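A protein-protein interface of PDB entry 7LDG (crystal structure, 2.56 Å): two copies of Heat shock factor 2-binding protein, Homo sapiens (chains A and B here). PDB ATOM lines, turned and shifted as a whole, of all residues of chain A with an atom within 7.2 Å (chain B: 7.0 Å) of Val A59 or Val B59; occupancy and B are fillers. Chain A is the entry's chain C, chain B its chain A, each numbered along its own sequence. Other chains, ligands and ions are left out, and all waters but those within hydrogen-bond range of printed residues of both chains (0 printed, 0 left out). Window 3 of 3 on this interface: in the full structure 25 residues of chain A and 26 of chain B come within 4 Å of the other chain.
The backbone carbonyl oxygen of Leu B50 lies close to the side-chain hydroxyl of Ser B54 (3.4 Å). OG of Ser B56 is in hydrogen-bond range of N of Val B59 (3.4 Å). The backbone carbonyl oxygen of Leu A50 is in hydrogen-bond range of the side-chain hydroxyl of Ser A54, 3.0 Å away. The side-chain hydroxyl (OG) of Ser A56 sits at hydrogen-bond distance from the backbone NH (N) of Val A59, at 3.2 Å.
Leu A49 touches Ile B63 (CD1 to CG2, 3.8 Å). Leu A50 touches Leu B50 (CG to CG, 3.9 Å). CG1 of Val A53 touches CB of Ala B62, at 3.8 Å. Val B53 touches Val A59 (CG1 to CG1, 3.8 Å). Val A59 touches Val B59. Val B53 touches Ala A62 (CG1 to CB, 3.8 Å). Ile A63 touches Leu B49 (CG2 to CD2, 3.8 Å).
Val A59 touches just these residues of chain B: Val B53 and Val B59. Of chain A, only Val A59 (3.7 Å) comes within 4 Å of Val B59. Of the printed residues of chain A, Val B53 touches Val A59 (3.8 Å) and Ala A62 (3.8 Å). Of the printed residues of chain B, Ala A62 touches Val B53 (3.8 Å). Glu B57 touches none of the printed residues of chain A. Gly A52 touches none of the printed residues of chain B. The nearest residue of chain B that does not touch Val A59 is Ser B56 (6.1 Å). The nearest printed residue of chain B that does not touch Leu A50 is Leu B49 (4.1 Å).
Printed residues of chain A that touch a printed residue of chain B: Leu A49, Leu A50, Val A53, Val A59, Ala A62 and Ile A63. Hydrophobic or aromatic side chains of chain B within 4 Å of the printed part of chain A: Leu B49, Leu B50, Val B53, Val B59, Ala B62 and Ile B63.
Leu B50 touches its own counterpart, Leu A50. Val A53 touches Ala B62, and with the chains exchanged Ala A62 touches Val B53. Val A59 touches Val B53, but with the chains exchanged Val A53 does not touch Val B59 (4.03 Å). Val B59 touches its own counterpart, Val A59.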
ATOM      1  N   LEU A  49     -19.167 -15.998  -5.933  1.00  0.00           N
ATOM      2  CA  LEU A  49     -19.431 -15.607  -7.313  1.00  0.00           C
ATOM      3  C   LEU A  49     -18.370 -16.166  -8.248  1.00  0.00           C
ATOM      4  O   LEU A  49     -18.693 -16.662  -9.333  1.00  0.00           O
ATOM      5  CB  LEU A  49     -19.507 -14.086  -7.428  1.00  0.00           C
ATOM      6  CG  LEU A  49     -20.723 -13.450  -6.756  1.00  0.00           C
ATOM      7  CD1 LEU A  49     -20.782 -11.961  -7.061  1.00  0.00           C
ATOM      8  CD2 LEU A  49     -22.008 -14.159  -7.184  1.00  0.00           C
ATOM      9  N   LEU A  50     -17.099 -16.097  -7.842  1.00  0.00           N
ATOM     10  CA  LEU A  50     -16.035 -16.723  -8.618  1.00  0.00           C
ATOM     11  C   LEU A  50     -16.263 -18.222  -8.737  1.00  0.00           C
ATOM     12  O   LEU A  50     -16.148 -18.795  -9.825  1.00  0.00           O
ATOM     13  CB  LEU A  50     -14.678 -16.440  -7.973  1.00  0.00           C
ATOM     14  CG  LEU A  50     -14.014 -15.107  -8.305  1.00  0.00           C
ATOM     15  CD1 LEU A  50     -12.780 -14.917  -7.443  1.00  0.00           C
ATOM     16  CD2 LEU A  50     -13.661 -15.065  -9.781  1.00  0.00           C
ATOM     17  N   GLY A  52     -18.991 -19.790  -8.782  1.00  0.00           N
ATOM     18  CA  GLY A  52     -20.063 -20.077  -9.723  1.00  0.00           C
ATOM     19  C   GLY A  52     -19.630 -19.946 -11.171  1.00  0.00           C
ATOM     20  O   GLY A  52     -19.844 -20.856 -11.978  1.00  0.00           O
ATOM     21  N   VAL A  53     -19.020 -18.810 -11.523  1.00  0.00           N
ATOM     22  CA  VAL A  53     -18.649 -18.577 -12.914  1.00  0.00           C
ATOM     23  C   VAL A  53     -17.450 -19.414 -13.339  1.00  0.00           C
ATOM     24  O   VAL A  53     -17.260 -19.639 -14.540  1.00  0.00           O
ATOM     25  CB  VAL A  53     -18.360 -17.087 -13.169  1.00  0.00           C
ATOM     26  CG1 VAL A  53     -19.597 -16.255 -12.893  1.00  0.00           C
ATOM     27  CG2 VAL A  53     -17.193 -16.619 -12.317  1.00  0.00           C
ATOM     28  N   SER A  54     -16.634 -19.888 -12.390  1.00  0.00           N
ATOM     29  CA  SER A  54     -15.442 -20.663 -12.725  1.00  0.00           C
ATOM     30  C   SER A  54     -15.760 -22.028 -13.323  1.00  0.00           C
ATOM     31  O   SER A  54     -14.827 -22.753 -13.686  1.00  0.00           O
ATOM     32  CB  SER A  54     -14.565 -20.845 -11.489  1.00  0.00           C
ATOM     33  OG  SER A  54     -15.232 -21.620 -10.516  1.00  0.00           O
ATOM     34  N   SER A  55     -17.034 -22.404 -13.425  1.00  0.00           N
ATOM     35  CA  SER A  55     -17.390 -23.641 -14.107  1.00  0.00           C
ATOM     36  C   SER A  55     -17.226 -23.522 -15.614  1.00  0.00           C
ATOM     37  O   SER A  55     -17.154 -24.545 -16.303  1.00  0.00           O
ATOM     38  CB  SER A  55     -18.823 -24.037 -13.765  1.00  0.00           C
ATOM     39  OG  SER A  55     -19.736 -23.043 -14.194  1.00  0.00           O
ATOM     40  N   SER A  56     -17.152 -22.305 -16.138  1.00  0.00           N
ATOM     41  CA  SER A  56     -16.936 -22.078 -17.559  1.00  0.00           C
ATOM     42  C   SER A  56     -15.448 -22.107 -17.876  1.00  0.00           C
ATOM     43  O   SER A  56     -14.634 -21.547 -17.138  1.00  0.00           O
ATOM     44  CB  SER A  56     -17.530 -20.737 -17.988  1.00  0.00           C
ATOM     45  OG  SER A  56     -16.751 -20.147 -19.007  1.00  0.00           O
ATOM     46  N   GLU A  57     -15.102 -22.763 -18.986  1.00  0.00           N
ATOM     47  CA  GLU A  57     -13.702 -22.853 -19.388  1.00  0.00           C
ATOM     48  C   GLU A  57     -13.154 -21.490 -19.798  1.00  0.00           C
ATOM     49  O   GLU A  57     -12.038 -21.121 -19.412  1.00  0.00           O
ATOM     50  CB  GLU A  57     -13.556 -23.855 -20.531  1.00  0.00           C
ATOM     51  CG  GLU A  57     -12.126 -24.076 -20.997  1.00  0.00           C
ATOM     52  CD  GLU A  57     -12.056 -24.953 -22.232  1.00  0.00           C
ATOM     53  OE1 GLU A  57     -10.997 -24.969 -22.896  1.00  0.00           O
ATOM     54  OE2 GLU A  57     -13.065 -25.620 -22.538  1.00  0.00           O
ATOM     55  N   GLU A  58     -13.928 -20.729 -20.580  1.00  0.00           N
ATOM     56  CA  GLU A  58     -13.482 -19.408 -21.013  1.00  0.00           C
ATOM     57  C   GLU A  58     -13.191 -18.503 -19.826  1.00  0.00           C
ATOM     58  O   GLU A  58     -12.238 -17.714 -19.859  1.00  0.00           O
ATOM     59  CB  GLU A  58     -14.533 -18.764 -21.916  1.00  0.00           C
ATOM     60  CG  GLU A  58     -14.742 -19.459 -23.247  1.00  0.00           C
ATOM     61  CD  GLU A  58     -15.899 -18.861 -24.029  1.00  0.00           C
ATOM     62  OE1 GLU A  58     -16.658 -18.053 -23.453  1.00  0.00           O
ATOM     63  OE2 GLU A  58     -16.050 -19.198 -25.220  1.00  0.00           O
ATOM     64  N   VAL A  59     -14.003 -18.597 -18.769  1.00  0.00           N
ATOM     65  CA  VAL A  59     -13.793 -17.762 -17.590  1.00  0.00           C
ATOM     66  C   VAL A  59     -12.484 -18.123 -16.905  1.00  0.00           C
ATOM     67  O   VAL A  59     -11.732 -17.242 -16.470  1.00  0.00           O
ATOM     68  CB  VAL A  59     -14.987 -17.888 -16.624  1.00  0.00           C
ATOM     69  CG1 VAL A  59     -14.708 -17.142 -15.338  1.00  0.00           C
ATOM     70  CG2 VAL A  59     -16.255 -17.362 -17.275  1.00  0.00           C
ATOM     71  N   VAL A  60     -12.190 -19.423 -16.795  1.00  0.00           N
ATOM     72  CA  VAL A  60     -10.947 -19.863 -16.165  1.00  0.00           C
ATOM     73  C   VAL A  60      -9.743 -19.345 -16.941  1.00  0.00           C
ATOM     74  O   VAL A  60      -8.757 -18.885 -16.351  1.00  0.00           O
ATOM     75  CB  VAL A  60     -10.927 -21.399 -16.037  1.00  0.00           C
ATOM     76  CG1 VAL A  60      -9.554 -21.885 -15.577  1.00  0.00           C
ATOM     77  CG2 VAL A  60     -11.992 -21.847 -15.061  1.00  0.00           C
ATOM     78  N   LYS A  61      -9.805 -19.406 -18.276  1.00  0.00           N
ATOM     79  CA  LYS A  61      -8.733 -18.841 -19.091  1.00  0.00           C
ATOM     80  C   LYS A  61      -8.549 -17.359 -18.796  1.00  0.00           C
ATOM     81  O   LYS A  61      -7.441 -16.909 -18.487  1.00  0.00           O
ATOM     82  CB  LYS A  61      -9.023 -19.058 -20.576  1.00  0.00           C
ATOM     83  CG  LYS A  61      -8.939 -20.505 -21.019  1.00  0.00           C
ATOM     84  CD  LYS A  61      -9.310 -20.661 -22.486  1.00  0.00           C
ATOM     85  CE  LYS A  61      -9.190 -22.110 -22.923  1.00  0.00           C
ATOM     86  NZ  LYS A  61      -9.700 -22.315 -24.304  1.00  0.00           N
ATOM     87  N   ALA A  62      -9.637 -16.589 -18.867  1.00  0.00           N
ATOM     88  CA  ALA A  62      -9.570 -15.157 -18.595  1.00  0.00           C
ATOM     89  C   ALA A  62      -8.973 -14.871 -17.223  1.00  0.00           C
ATOM     90  O   ALA A  62      -8.161 -13.952 -17.073  1.00  0.00           O
ATOM     91  CB  ALA A  62     -10.965 -14.542 -18.714  1.00  0.00           C
ATOM     92  N   ILE A  63      -9.353 -15.654 -16.214  1.00  0.00           N
ATOM     93  CA  ILE A  63      -8.821 -15.447 -14.869  1.00  0.00           C
ATOM     94  C   ILE A  63      -7.308 -15.614 -14.865  1.00  0.00           C
ATOM     95  O   ILE A  63      -6.571 -14.798 -14.299  1.00  0.00           O
ATOM     96  CB  ILE A  63      -9.490 -16.408 -13.872  1.00  0.00           C
ATOM     97  CG1 ILE A  63     -10.942 -15.999 -13.623  1.00  0.00           C
ATOM     98  CG2 ILE A  63      -8.704 -16.459 -12.574  1.00  0.00           C
ATOM     99  CD1 ILE A  63     -11.626 -16.845 -12.573  1.00  0.00           C
ATOM    100  N   LEU A  64      -6.821 -16.678 -15.500  1.00  0.00           N
ATOM    101  CA  LEU A  64      -5.390 -16.953 -15.484  1.00  0.00           C
ATOM    102  C   LEU A  64      -4.595 -15.940 -16.300  1.00  0.00           C
ATOM    103  O   LEU A  64      -3.395 -15.774 -16.050  1.00  0.00           O
ATOM    104  CB  LEU A  64      -5.125 -18.366 -15.999  1.00  0.00           C
ATOM    105  CG  LEU A  64      -5.834 -19.462 -15.192  1.00  0.00           C
ATOM    106  CD1 LEU A  64      -5.583 -20.840 -15.779  1.00  0.00           C
ATOM    107  CD2 LEU A  64      -5.414 -19.410 -13.733  1.00  0.00           C
ATOM    108  N   GLY A  65      -5.228 -15.257 -17.258  1.00  0.00           N
ATOM    109  CA  GLY A  65      -4.535 -14.237 -18.038  1.00  0.00           C
ATOM    110  C   GLY A  65      -4.358 -12.906 -17.333  1.00  0.00           C
ATOM    111  O   GLY A  65      -3.750 -11.998 -17.911  1.00  0.00           O
ATOM    112  N   LEU B  49     -10.301 -10.198 -10.447  1.00  0.00           N
ATOM    113  CA  LEU B  49     -10.670 -11.326 -11.296  1.00  0.00           C
ATOM    114  C   LEU B  49     -12.127 -11.223 -11.728  1.00  0.00           C
ATOM    115  O   LEU B  49     -12.453 -11.429 -12.904  1.00  0.00           O
ATOM    116  CB  LEU B  49     -10.414 -12.643 -10.559  1.00  0.00           C
ATOM    117  CG  LEU B  49      -8.964 -12.929 -10.160  1.00  0.00           C
ATOM    118  CD1 LEU B  49      -8.859 -14.237  -9.393  1.00  0.00           C
ATOM    119  CD2 LEU B  49      -8.066 -12.956 -11.387  1.00  0.00           C
ATOM    120  N   LEU B  50     -13.013 -10.881 -10.789  1.00  0.00           N
ATOM    121  CA  LEU B  50     -14.425 -10.712 -11.120  1.00  0.00           C
ATOM    122  C   LEU B  50     -14.628  -9.565 -12.100  1.00  0.00           C
ATOM    123  O   LEU B  50     -15.359  -9.705 -13.089  1.00  0.00           O
ATOM    124  CB  LEU B  50     -15.232 -10.480  -9.844  1.00  0.00           C
ATOM    125  CG  LEU B  50     -15.838 -11.734  -9.219  1.00  0.00           C
ATOM    126  CD1 LEU B  50     -16.483 -11.409  -7.880  1.00  0.00           C
ATOM    127  CD2 LEU B  50     -16.845 -12.337 -10.183  1.00  0.00           C
ATOM    128  N   GLY B  52     -12.497  -8.482 -14.205  1.00  0.00           N
ATOM    129  CA  GLY B  52     -11.971  -8.919 -15.489  1.00  0.00           C
ATOM    130  C   GLY B  52     -12.980  -9.690 -16.320  1.00  0.00           C
ATOM    131  O   GLY B  52     -13.114  -9.455 -17.522  1.00  0.00           O
ATOM    132  N   VAL B  53     -13.716 -10.612 -15.692  1.00  0.00           N
ATOM    133  CA  VAL B  53     -14.648 -11.454 -16.442  1.00  0.00           C
ATOM    134  C   VAL B  53     -16.051 -10.867 -16.542  1.00  0.00           C
ATOM    135  O   VAL B  53     -16.872 -11.384 -17.315  1.00  0.00           O
ATOM    136  CB  VAL B  53     -14.731 -12.867 -15.827  1.00  0.00           C
ATOM    137  CG1 VAL B  53     -13.395 -13.577 -15.961  1.00  0.00           C
ATOM    138  CG2 VAL B  53     -15.127 -12.790 -14.372  1.00  0.00           C
ATOM    139  N   SER B  54     -16.353  -9.793 -15.807  1.00  0.00           N
ATOM    140  CA  SER B  54     -17.708  -9.247 -15.810  1.00  0.00           C
ATOM    141  C   SER B  54     -18.076  -8.571 -17.125  1.00  0.00           C
ATOM    142  O   SER B  54     -19.245  -8.211 -17.310  1.00  0.00           O
ATOM    143  CB  SER B  54     -17.887  -8.259 -14.654  1.00  0.00           C
ATOM    144  OG  SER B  54     -16.934  -7.213 -14.725  1.00  0.00           O
ATOM    145  N   SER B  55     -17.122  -8.395 -18.042  1.00  0.00           N
ATOM    146  CA  SER B  55     -17.447  -7.880 -19.368  1.00  0.00           C
ATOM    147  C   SER B  55     -18.278  -8.854 -20.191  1.00  0.00           C
ATOM    148  O   SER B  55     -18.800  -8.461 -21.240  1.00  0.00           O
ATOM    149  CB  SER B  55     -16.167  -7.535 -20.128  1.00  0.00           C
ATOM    150  OG  SER B  55     -15.208  -8.568 -19.997  1.00  0.00           O
ATOM    151  N   SER B  56     -18.414 -10.101 -19.744  1.00  0.00           N
ATOM    152  CA  SER B  56     -19.187 -11.111 -20.454  1.00  0.00           C
ATOM    153  C   SER B  56     -20.646 -11.072 -20.016  1.00  0.00           C
ATOM    154  O   SER B  56     -20.942 -11.086 -18.817  1.00  0.00           O
ATOM    155  CB  SER B  56     -18.608 -12.502 -20.194  1.00  0.00           C
ATOM    156  OG  SER B  56     -19.483 -13.513 -20.663  1.00  0.00           O
ATOM    157  N   GLU B  57     -21.555 -11.048 -20.991  1.00  0.00           N
ATOM    158  CA  GLU B  57     -22.976 -11.106 -20.662  1.00  0.00           C
ATOM    159  C   GLU B  57     -23.311 -12.367 -19.875  1.00  0.00           C
ATOM    160  O   GLU B  57     -24.078 -12.318 -18.906  1.00  0.00           O
ATOM    161  CB  GLU B  57     -23.819 -11.031 -21.933  1.00  0.00           C
ATOM    162  CG  GLU B  57     -25.315 -11.143 -21.676  1.00  0.00           C
ATOM    163  CD  GLU B  57     -26.148 -10.650 -22.843  1.00  0.00           C
ATOM    164  OE1 GLU B  57     -25.558 -10.269 -23.877  1.00  0.00           O
ATOM    165  OE2 GLU B  57     -27.392 -10.639 -22.723  1.00  0.00           O
ATOM    166  N   GLU B  58     -22.734 -13.505 -20.267  1.00  0.00           N
ATOM    167  CA  GLU B  58     -23.028 -14.751 -19.568  1.00  0.00           C
ATOM    168  C   GLU B  58     -22.487 -14.735 -18.148  1.00  0.00           C
ATOM    169  O   GLU B  58     -23.093 -15.329 -17.251  1.00  0.00           O
ATOM    170  CB  GLU B  58     -22.476 -15.943 -20.352  1.00  0.00           C
ATOM    171  CG  GLU B  58     -23.352 -16.329 -21.548  1.00  0.00           C
ATOM    172  CD  GLU B  58     -24.821 -16.523 -21.164  1.00  0.00           C
ATOM    173  OE1 GLU B  58     -25.097 -17.145 -20.111  1.00  0.00           O
ATOM    174  OE2 GLU B  58     -25.700 -16.045 -21.915  1.00  0.00           O
ATOM    175  N   VAL B  59     -21.369 -14.048 -17.915  1.00  0.00           N
ATOM    176  CA  VAL B  59     -20.858 -13.938 -16.553  1.00  0.00           C
ATOM    177  C   VAL B  59     -21.786 -13.077 -15.704  1.00  0.00           C
ATOM    178  O   VAL B  59     -22.056 -13.391 -14.536  1.00  0.00           O
ATOM    179  CB  VAL B  59     -19.420 -13.390 -16.570  1.00  0.00           C
ATOM    180  CG1 VAL B  59     -18.981 -12.989 -15.169  1.00  0.00           C
ATOM    181  CG2 VAL B  59     -18.475 -14.428 -17.143  1.00  0.00           C
ATOM    182  N   VAL B  60     -22.299 -11.986 -16.276  1.00  0.00           N
ATOM    183  CA  VAL B  60     -23.213 -11.117 -15.538  1.00  0.00           C
ATOM    184  C   VAL B  60     -24.470 -11.886 -15.160  1.00  0.00           C
ATOM    185  O   VAL B  60     -24.893 -11.886 -13.999  1.00  0.00           O
ATOM    186  CB  VAL B  60     -23.548  -9.859 -16.361  1.00  0.00           C
ATOM    187  CG1 VAL B  60     -24.697  -9.093 -15.720  1.00  0.00           C
ATOM    188  CG2 VAL B  60     -22.321  -8.970 -16.511  1.00  0.00           C
ATOM    189  N   LYS B  61     -25.079 -12.562 -16.136  1.00  0.00           N
ATOM    190  CA  LYS B  61     -26.261 -13.376 -15.867  1.00  0.00           C
ATOM    191  C   LYS B  61     -25.983 -14.399 -14.775  1.00  0.00           C
ATOM    192  O   LYS B  61     -26.787 -14.581 -13.854  1.00  0.00           O
ATOM    193  CB  LYS B  61     -26.722 -14.071 -17.148  1.00  0.00           C
ATOM    194  CG  LYS B  61     -27.277 -13.127 -18.204  1.00  0.00           C
ATOM    195  CD  LYS B  61     -27.583 -13.857 -19.494  1.00  0.00           C
ATOM    196  CE  LYS B  61     -28.367 -12.974 -20.445  1.00  0.00           C
ATOM    197  NZ  LYS B  61     -28.745 -13.701 -21.689  1.00  0.00           N
ATOM    198  N   ALA B  62     -24.829 -15.062 -14.852  1.00  0.00           N
ATOM    199  CA  ALA B  62     -24.455 -16.017 -13.815  1.00  0.00           C
ATOM    200  C   ALA B  62     -24.338 -15.341 -12.453  1.00  0.00           C
ATOM    201  O   ALA B  62     -24.778 -15.896 -11.439  1.00  0.00           O
ATOM    202  CB  ALA B  62     -23.146 -16.707 -14.193  1.00  0.00           C
ATOM    203  N   ILE B  63     -23.749 -14.144 -12.406  1.00  0.00           N
ATOM    204  CA  ILE B  63     -23.602 -13.438 -11.133  1.00  0.00           C
ATOM    205  C   ILE B  63     -24.967 -13.130 -10.533  1.00  0.00           C
ATOM    206  O   ILE B  63     -25.209 -13.364  -9.344  1.00  0.00           O
ATOM    207  CB  ILE B  63     -22.774 -12.155 -11.321  1.00  0.00           C
ATOM    208  CG1 ILE B  63     -21.311 -12.490 -11.596  1.00  0.00           C
ATOM    209  CG2 ILE B  63     -22.884 -11.263 -10.100  1.00  0.00           C
ATOM    210  CD1 ILE B  63     -20.453 -11.264 -11.778  1.00  0.00           C
ATOM    211  N   LEU B  64     -25.879 -12.600 -11.349  1.00  0.00           N
ATOM    212  CA  LEU B  64     -27.214 -12.266 -10.863  1.00  0.00           C
ATOM    213  C   LEU B  64     -27.952 -13.483 -10.322  1.00  0.00           C
ATOM    214  O   LEU B  64     -28.879 -13.325  -9.518  1.00  0.00           O
ATOM    215  CB  LEU B  64     -28.026 -11.608 -11.981  1.00  0.00           C
ATOM    216  CG  LEU B  64     -27.384 -10.333 -12.536  1.00  0.00           C
ATOM    217  CD1 LEU B  64     -28.224  -9.714 -13.639  1.00  0.00           C
ATOM    218  CD2 LEU B  64     -27.125  -9.324 -11.422  1.00  0.00           C
ATOM    219  N   GLY B  65     -27.553 -14.685 -10.730  1.00  0.00           N
ATOM    220  CA  GLY B  65     -28.168 -15.904 -10.249  1.00  0.00           C
ATOM    221  C   GLY B  65     -28.064 -16.099  -8.751  1.00  0.00           C
ATOM    222  O   GLY B  65     -26.967 -16.236  -8.200  1.00  0.00           O
